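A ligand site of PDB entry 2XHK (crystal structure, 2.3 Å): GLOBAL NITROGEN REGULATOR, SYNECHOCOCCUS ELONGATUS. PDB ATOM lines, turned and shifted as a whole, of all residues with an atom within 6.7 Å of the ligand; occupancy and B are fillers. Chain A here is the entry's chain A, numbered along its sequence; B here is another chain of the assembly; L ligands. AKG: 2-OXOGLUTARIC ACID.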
ATOM      1  N   PHE A  34       9.190 -28.326 -24.114  1.00  0.00           N
ATOM      2  CA  PHE A  34      10.384 -29.197 -24.116  1.00  0.00           C
ATOM      3  C   PHE A  34      10.069 -30.585 -23.590  1.00  0.00           C
ATOM      4  O   PHE A  34       9.148 -30.755 -22.805  1.00  0.00           O
ATOM      5  CB  PHE A  34      11.611 -28.557 -23.387  1.00  0.00           C
ATOM      6  CG  PHE A  34      11.379 -28.187 -21.937  1.00  0.00           C
ATOM      7  CD1 PHE A  34      11.220 -29.154 -20.964  1.00  0.00           C
ATOM      8  CD2 PHE A  34      11.397 -26.844 -21.548  1.00  0.00           C
ATOM      9  CE1 PHE A  34      11.042 -28.799 -19.614  1.00  0.00           C
ATOM     10  CE2 PHE A  34      11.225 -26.478 -20.203  1.00  0.00           C
ATOM     11  CZ  PHE A  34      11.027 -27.456 -19.244  1.00  0.00           C
ATOM     12  N   ALA A  40      19.196 -28.794 -21.734  1.00  0.00           N
ATOM     13  CA  ALA A  40      18.638 -27.685 -20.957  1.00  0.00           C
ATOM     14  C   ALA A  40      19.516 -26.479 -21.261  1.00  0.00           C
ATOM     15  O   ALA A  40      20.385 -26.120 -20.474  1.00  0.00           O
ATOM     16  CB  ALA A  40      18.648 -28.024 -19.451  1.00  0.00           C
ATOM     17  N   ARG A  42      18.092 -23.364 -22.616  1.00  0.00           N
ATOM     18  CA  ARG A  42      17.322 -22.123 -22.666  1.00  0.00           C
ATOM     19  C   ARG A  42      16.594 -21.838 -21.368  1.00  0.00           C
ATOM     20  O   ARG A  42      16.274 -22.741 -20.615  1.00  0.00           O
ATOM     21  CB  ARG A  42      16.295 -22.150 -23.807  1.00  0.00           C
ATOM     22  CG  ARG A  42      16.930 -22.173 -25.159  1.00  0.00           C
ATOM     23  CD  ARG A  42      15.937 -22.081 -26.341  1.00  0.00           C
ATOM     24  NE  ARG A  42      16.721 -21.678 -27.503  1.00  0.00           N
ATOM     25  CZ  ARG A  42      16.639 -20.513 -28.132  1.00  0.00           C
ATOM     26  NH1 ARG A  42      15.736 -19.603 -27.815  1.00  0.00           N
ATOM     27  NH2 ARG A  42      17.461 -20.283 -29.131  1.00  0.00           N
ATOM     28  N   LEU A  53       4.145 -28.369 -16.233  1.00  0.00           N
ATOM     29  CA  LEU A  53       5.403 -29.105 -16.056  1.00  0.00           C
ATOM     30  C   LEU A  53       5.004 -30.397 -15.387  1.00  0.00           C
ATOM     31  O   LEU A  53       4.307 -30.389 -14.384  1.00  0.00           O
ATOM     32  CB  LEU A  53       6.376 -28.347 -15.153  1.00  0.00           C
ATOM     33  CG  LEU A  53       7.001 -27.021 -15.610  1.00  0.00           C
ATOM     34  CD1 LEU A  53       8.105 -26.565 -14.617  1.00  0.00           C
ATOM     35  CD2 LEU A  53       7.587 -27.146 -17.031  1.00  0.00           C
ATOM     36  N   VAL A  65       3.785 -31.307 -11.720  1.00  0.00           N
ATOM     37  CA  VAL A  65       4.696 -30.745 -10.748  1.00  0.00           C
ATOM     38  C   VAL A  65       4.523 -29.218 -10.656  1.00  0.00           C
ATOM     39  O   VAL A  65       4.835 -28.636  -9.641  1.00  0.00           O
ATOM     40  CB  VAL A  65       6.121 -31.111 -11.188  1.00  0.00           C
ATOM     41  CG1 VAL A  65       7.085 -30.052 -10.827  1.00  0.00           C
ATOM     42  CG2 VAL A  65       6.535 -32.557 -10.691  1.00  0.00           C
ATOM     43  N   ALA A  66       4.053 -28.572 -11.737  1.00  0.00           N
ATOM     44  CA  ALA A  66       3.774 -27.120 -11.725  1.00  0.00           C
ATOM     45  C   ALA A  66       2.777 -26.730 -12.798  1.00  0.00           C
ATOM     46  O   ALA A  66       2.795 -27.288 -13.895  1.00  0.00           O
ATOM     47  CB  ALA A  66       5.057 -26.299 -11.905  1.00  0.00           C
ATOM     48  N   LEU A  68       2.108 -23.299 -14.338  1.00  0.00           N
ATOM     49  CA  LEU A  68       2.792 -22.030 -14.327  1.00  0.00           C
ATOM     50  C   LEU A  68       1.866 -20.934 -14.870  1.00  0.00           C
ATOM     51  O   LEU A  68       1.145 -21.149 -15.846  1.00  0.00           O
ATOM     52  CB  LEU A  68       4.058 -22.081 -15.196  1.00  0.00           C
ATOM     53  CG  LEU A  68       5.147 -23.076 -14.784  1.00  0.00           C
ATOM     54  CD1 LEU A  68       6.238 -23.168 -15.854  1.00  0.00           C
ATOM     55  CD2 LEU A  68       5.732 -22.769 -13.437  1.00  0.00           C
ATOM     56  N   VAL A  73       9.146 -17.150 -14.859  1.00  0.00           N
ATOM     57  CA  VAL A  73      10.389 -17.677 -15.428  1.00  0.00           C
ATOM     58  C   VAL A  73      10.419 -19.196 -15.263  1.00  0.00           C
ATOM     59  O   VAL A  73       9.978 -19.701 -14.231  1.00  0.00           O
ATOM     60  CB  VAL A  73      11.597 -17.035 -14.736  1.00  0.00           C
ATOM     61  CG1 VAL A  73      12.887 -17.396 -15.439  1.00  0.00           C
ATOM     62  CG2 VAL A  73      11.452 -15.506 -14.702  1.00  0.00           C
ATOM     63  N   PHE A  74      10.887 -19.934 -16.266  1.00  0.00           N
ATOM     64  CA  PHE A  74      11.003 -21.393 -16.131  1.00  0.00           C
ATOM     65  C   PHE A  74      12.056 -21.958 -17.063  1.00  0.00           C
ATOM     66  O   PHE A  74      12.716 -21.219 -17.820  1.00  0.00           O
ATOM     67  CB  PHE A  74       9.630 -22.120 -16.266  1.00  0.00           C
ATOM     68  CG  PHE A  74       9.036 -22.113 -17.663  1.00  0.00           C
ATOM     69  CD1 PHE A  74       9.097 -23.246 -18.482  1.00  0.00           C
ATOM     70  CD2 PHE A  74       8.388 -20.985 -18.164  1.00  0.00           C
ATOM     71  CE1 PHE A  74       8.560 -23.246 -19.770  1.00  0.00           C
ATOM     72  CE2 PHE A  74       7.845 -20.977 -19.462  1.00  0.00           C
ATOM     73  CZ  PHE A  74       7.927 -22.103 -20.259  1.00  0.00           C
ATOM     74  N   GLY A  75      12.248 -23.281 -17.015  1.00  0.00           N
ATOM     75  CA  GLY A  75      13.358 -23.905 -17.726  1.00  0.00           C
ATOM     76  C   GLY A  75      14.612 -23.724 -16.882  1.00  0.00           C
ATOM     77  O   GLY A  75      15.756 -23.791 -17.351  1.00  0.00           O
ATOM     78  N   VAL A  76      14.364 -23.568 -15.592  1.00  0.00           N
ATOM     79  CA  VAL A  76      15.374 -23.089 -14.661  1.00  0.00           C
ATOM     80  C   VAL A  76      16.589 -24.022 -14.491  1.00  0.00           C
ATOM     81  O   VAL A  76      17.641 -23.591 -13.985  1.00  0.00           O
ATOM     82  CB  VAL A  76      14.616 -22.776 -13.321  1.00  0.00           C
ATOM     83  CG1 VAL A  76      15.189 -23.516 -12.190  1.00  0.00           C
ATOM     84  CG2 VAL A  76      14.430 -21.266 -13.152  1.00  0.00           C
ATOM     85  N   LEU A  77      16.480 -25.278 -14.934  1.00  0.00           N
ATOM     86  CA  LEU A  77      17.618 -26.220 -14.872  1.00  0.00           C
ATOM     87  C   LEU A  77      18.823 -25.688 -15.652  1.00  0.00           C
ATOM     88  O   LEU A  77      19.959 -25.930 -15.272  1.00  0.00           O
ATOM     89  CB  LEU A  77      17.241 -27.587 -15.457  1.00  0.00           C
ATOM     90  CG  LEU A  77      18.307 -28.665 -15.569  1.00  0.00           C
ATOM     91  CD1 LEU A  77      18.904 -28.982 -14.177  1.00  0.00           C
ATOM     92  CD2 LEU A  77      17.756 -29.948 -16.237  1.00  0.00           C
ATOM     93  N   SER A  78      18.532 -24.967 -16.732  1.00  0.00           N
ATOM     94  CA  SER A  78      19.523 -24.395 -17.622  1.00  0.00           C
ATOM     95  C   SER A  78      20.485 -23.451 -16.910  1.00  0.00           C
ATOM     96  O   SER A  78      21.635 -23.304 -17.326  1.00  0.00           O
ATOM     97  CB  SER A  78      18.809 -23.663 -18.786  1.00  0.00           C
ATOM     98  OG  SER A  78      18.017 -22.548 -18.328  1.00  0.00           O
ATOM     99  N   ASP A  86      20.293 -32.867 -19.194  1.00  0.00           N
ATOM    100  CA  ASP A  86      19.086 -32.976 -19.940  1.00  0.00           C
ATOM    101  C   ASP A  86      17.864 -32.697 -19.072  1.00  0.00           C
ATOM    102  O   ASP A  86      17.808 -33.019 -17.888  1.00  0.00           O
ATOM    103  CB  ASP A  86      19.053 -34.358 -20.618  1.00  0.00           C
ATOM    104  CG  ASP A  86      20.205 -34.543 -21.630  1.00  0.00           C
ATOM    105  OD1 ASP A  86      20.683 -33.532 -22.189  1.00  0.00           O
ATOM    106  OD2 ASP A  86      20.643 -35.697 -21.880  1.00  0.00           O
ATOM    107  N   ARG A  87      16.908 -32.017 -19.684  1.00  0.00           N
ATOM    108  CA  ARG A  87      15.559 -31.937 -19.187  1.00  0.00           C
ATOM    109  C   ARG A  87      15.079 -33.295 -18.680  1.00  0.00           C
ATOM    110  O   ARG A  87      15.294 -34.283 -19.342  1.00  0.00           O
ATOM    111  CB  ARG A  87      14.656 -31.520 -20.332  1.00  0.00           C
ATOM    112  CG  ARG A  87      14.132 -30.154 -20.254  1.00  0.00           C
ATOM    113  CD  ARG A  87      14.943 -29.017 -20.804  1.00  0.00           C
ATOM    114  NE  ARG A  87      15.027 -28.074 -19.734  1.00  0.00           N
ATOM    115  CZ  ARG A  87      15.270 -26.775 -19.768  1.00  0.00           C
ATOM    116  NH1 ARG A  87      15.476 -26.128 -20.866  1.00  0.00           N
ATOM    117  NH2 ARG A  87      15.334 -26.137 -18.591  1.00  0.00           N
ATOM    118  N   PHE A  88      14.441 -33.319 -17.507  1.00  0.00           N
ATOM    119  CA  PHE A  88      13.751 -34.513 -17.013  1.00  0.00           C
ATOM    120  C   PHE A  88      12.247 -34.299 -16.786  1.00  0.00           C
ATOM    121  O   PHE A  88      11.526 -35.248 -16.475  1.00  0.00           O
ATOM    122  CB  PHE A  88      14.408 -35.052 -15.727  1.00  0.00           C
ATOM    123  CG  PHE A  88      14.666 -33.996 -14.695  1.00  0.00           C
ATOM    124  CD1 PHE A  88      13.660 -33.621 -13.814  1.00  0.00           C
ATOM    125  CD2 PHE A  88      15.926 -33.373 -14.597  1.00  0.00           C
ATOM    126  CE1 PHE A  88      13.862 -32.616 -12.845  1.00  0.00           C
ATOM    127  CE2 PHE A  88      16.165 -32.370 -13.646  1.00  0.00           C
ATOM    128  CZ  PHE A  88      15.113 -31.994 -12.743  1.00  0.00           C
ATOM    129  N   TYR A  89      11.761 -33.055 -16.904  1.00  0.00           N
ATOM    130  CA  TYR A  89      10.337 -32.815 -16.956  1.00  0.00           C
ATOM    131  C   TYR A  89       9.893 -32.526 -18.392  1.00  0.00           C
ATOM    132  O   TYR A  89      10.684 -32.168 -19.267  1.00  0.00           O
ATOM    133  CB  TYR A  89       9.924 -31.659 -16.055  1.00  0.00           C
ATOM    134  CG  TYR A  89      10.093 -31.896 -14.533  1.00  0.00           C
ATOM    135  CD1 TYR A  89       9.900 -33.146 -13.981  1.00  0.00           C
ATOM    136  CD2 TYR A  89      10.408 -30.831 -13.675  1.00  0.00           C
ATOM    137  CE1 TYR A  89      10.052 -33.360 -12.614  1.00  0.00           C
ATOM    138  CE2 TYR A  89      10.546 -31.007 -12.321  1.00  0.00           C
ATOM    139  CZ  TYR A  89      10.370 -32.287 -11.793  1.00  0.00           C
ATOM    140  OH  TYR A  89      10.490 -32.499 -10.444  1.00  0.00           O
ATOM    141  N   HIS A  90       8.590 -32.682 -18.588  1.00  0.00           N
ATOM    142  CA  HIS A  90       7.890 -32.397 -19.813  1.00  0.00           C
ATOM    143  C   HIS A  90       7.149 -31.066 -19.637  1.00  0.00           C
ATOM    144  O   HIS A  90       6.338 -30.917 -18.711  1.00  0.00           O
ATOM    145  CB  HIS A  90       6.916 -33.540 -20.050  1.00  0.00           C
ATOM    146  CG  HIS A  90       6.199 -33.483 -21.355  1.00  0.00           C
ATOM    147  ND1 HIS A  90       5.011 -34.140 -21.569  1.00  0.00           N
ATOM    148  CD2 HIS A  90       6.500 -32.849 -22.517  1.00  0.00           C
ATOM    149  CE1 HIS A  90       4.610 -33.927 -22.819  1.00  0.00           C
ATOM    150  NE2 HIS A  90       5.494 -33.138 -23.411  1.00  0.00           N
ATOM    151  N   ALA A  91       7.449 -30.084 -20.487  1.00  0.00           N
ATOM    152  CA  ALA A  91       6.731 -28.811 -20.445  1.00  0.00           C
ATOM    153  C   ALA A  91       5.800 -28.706 -21.658  1.00  0.00           C
ATOM    154  O   ALA A  91       6.246 -28.821 -22.813  1.00  0.00           O
ATOM    155  CB  ALA A  91       7.700 -27.611 -20.374  1.00  0.00           C
ATOM    156  N   ARG A 128       8.814 -18.204  -7.724  1.00  0.00           N
ATOM    157  CA  ARG A 128       8.616 -19.601  -8.107  1.00  0.00           C
ATOM    158  C   ARG A 128       8.767 -20.533  -6.916  1.00  0.00           C
ATOM    159  O   ARG A 128       7.969 -21.454  -6.766  1.00  0.00           O
ATOM    160  CB  ARG A 128       9.616 -20.047  -9.184  1.00  0.00           C
ATOM    161  CG  ARG A 128       9.377 -19.393 -10.590  1.00  0.00           C
ATOM    162  CD  ARG A 128       8.118 -19.906 -11.307  1.00  0.00           C
ATOM    163  NE  ARG A 128       7.995 -21.353 -11.186  1.00  0.00           N
ATOM    164  CZ  ARG A 128       8.810 -22.232 -11.727  1.00  0.00           C
ATOM    165  NH1 ARG A 128       9.837 -21.834 -12.463  1.00  0.00           N
ATOM    166  NH2 ARG A 128       8.622 -23.523 -11.518  1.00  0.00           N
ATOM    167  N   THR A 132       5.861 -22.846  -5.573  1.00  0.00           N
ATOM    168  CA  THR A 132       6.003 -24.318  -5.414  1.00  0.00           C
ATOM    169  C   THR A 132       5.691 -24.794  -3.965  1.00  0.00           C
ATOM    170  O   THR A 132       5.040 -25.837  -3.734  1.00  0.00           O
ATOM    171  CB  THR A 132       7.368 -24.792  -5.860  1.00  0.00           C
ATOM    172  OG1 THR A 132       7.693 -24.179  -7.096  1.00  0.00           O
ATOM    173  CG2 THR A 132       7.389 -26.286  -6.078  1.00  0.00           C
ATOM    174  N   ILE B 129      14.199 -24.455  -6.466  1.00  0.00           N
ATOM    175  CA  ILE B 129      12.977 -24.746  -7.246  1.00  0.00           C
ATOM    176  C   ILE B 129      12.899 -26.234  -7.588  1.00  0.00           C
ATOM    177  O   ILE B 129      11.889 -26.874  -7.294  1.00  0.00           O
ATOM    178  CB  ILE B 129      12.934 -23.900  -8.549  1.00  0.00           C
ATOM    179  CG1 ILE B 129      12.801 -22.413  -8.197  1.00  0.00           C
ATOM    180  CG2 ILE B 129      11.763 -24.379  -9.483  1.00  0.00           C
ATOM    181  CD1 ILE B 129      12.943 -21.439  -9.399  1.00  0.00           C
ATOM    182  N   LEU B 130      13.989 -26.756  -8.142  1.00  0.00           N
ATOM    183  CA  LEU B 130      14.097 -28.176  -8.473  1.00  0.00           C
ATOM    184  C   LEU B 130      13.909 -29.118  -7.256  1.00  0.00           C
ATOM    185  O   LEU B 130      13.220 -30.128  -7.374  1.00  0.00           O
ATOM    186  CB  LEU B 130      15.443 -28.490  -9.157  1.00  0.00           C
ATOM    187  CG  LEU B 130      15.695 -27.770 -10.493  1.00  0.00           C
ATOM    188  CD1 LEU B 130      17.104 -28.110 -11.066  1.00  0.00           C
ATOM    189  CD2 LEU B 130      14.587 -28.007 -11.563  1.00  0.00           C
ATOM    190  N   GLU B 133      10.210 -29.103  -6.243  1.00  0.00           N
ATOM    191  CA  GLU B 133       9.488 -29.909  -7.232  1.00  0.00           C
ATOM    192  C   GLU B 133       9.656 -31.410  -7.013  1.00  0.00           C
ATOM    193  O   GLU B 133       8.679 -32.155  -7.185  1.00  0.00           O
ATOM    194  CB  GLU B 133       9.869 -29.509  -8.688  1.00  0.00           C
ATOM    195  CG  GLU B 133       9.336 -28.134  -9.069  1.00  0.00           C
ATOM    196  CD  GLU B 133       9.864 -27.580 -10.377  1.00  0.00           C
ATOM    197  OE1 GLU B 133      10.941 -28.010 -10.898  1.00  0.00           O
ATOM    198  OE2 GLU B 133       9.178 -26.669 -10.883  1.00  0.00           O
HETATM  199  C1  AKG L   1      13.750 -28.319 -16.335  1.00  0.00           C
HETATM  200  O1  AKG L   1      14.728 -28.170 -17.064  1.00  0.00           O
HETATM  201  O2  AKG L   1      13.067 -29.331 -16.265  1.00  0.00           O
HETATM  202  C2  AKG L   1      13.421 -27.256 -15.443  1.00  0.00           C
HETATM  203  O5  AKG L   1      14.154 -26.298 -15.571  1.00  0.00           O
HETATM  204  C3  AKG L   1      12.177 -27.277 -14.514  1.00  0.00           C
HETATM  205  C4  AKG L   1      11.239 -26.090 -14.935  1.00  0.00           C
HETATM  206  C5  AKG L   1      11.102 -24.943 -13.858  1.00  0.00           C
HETATM  207  O3  AKG L   1      11.558 -23.841 -14.155  1.00  0.00           O
HETATM  208  O4  AKG L   1      10.445 -25.116 -12.803  1.00  0.00           O
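NH2 of Arg 87 sits at hydrogen-bond distance from O of Gly 75, at 2.7 Å. NH1 of Arg 87 is in hydrogen-bond range of O of Arg 42 (3.5 Å). The side-chain carboxylate (OE2) of Glu 133 of chain B lies within salt-bridge range of the guanidinium group (NH2) of Arg 128 (3.3 Å). O of Val 73 sits at hydrogen-bond distance from NH1 of Arg 128, 2.8 Å away. OG1 of Thr 132 sits at hydrogen-bond distance from O of Arg 128, 2.8 Å away. The side-chain hydroxyl of Ser 78 sits at hydrogen-bond distance from the backbone carbonyl oxygen of Gly 75, at 2.8 Å. The backbone carbonyl oxygen (O) of Ala 66 lies within hydrogen-bond range of the backbone NH (N) of Leu 53 (2.9 Å). The backbone carbonyl oxygen (O) of Leu 53 lies within hydrogen-bond range of the backbone NH (N) of Val 65, 2.9 Å away.
Merely in contact with the ligand: Phe 34, Leu 53, Phe 74, Tyr 89, Ile 129 of chain B and Leu 130 of chain B. Hydrophobic or aromatic side chains that line the ligand: Phe 34, Leu 53, Phe 74, Val 76, Leu 77, Tyr 89, Ile 129 of chain B and Leu 130 of chain B.
The guanidinium group of Arg 87 lies within salt-bridge range of an oxygen (O1) of the ligand (2.6 Å). The backbone NH of Leu 77 is in hydrogen-bond range of an oxygen (O5) of the ligand (2.6 Å). An oxygen (O5) of the ligand sits at hydrogen-bond distance from the backbone NH (N) of Val 76, at 2.7 Å. An oxygen (O4) of the ligand lies within salt-bridge range of the guanidinium group (NH2) of Arg 128 (2.7 Å). The side-chain carboxylate of Glu 133 of chain B sits close to an oxygen (O4) of the ligand, 2.8 Å away. N of Gly 75 lies within hydrogen-bond range of O3 of the ligand (3.0 Å).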
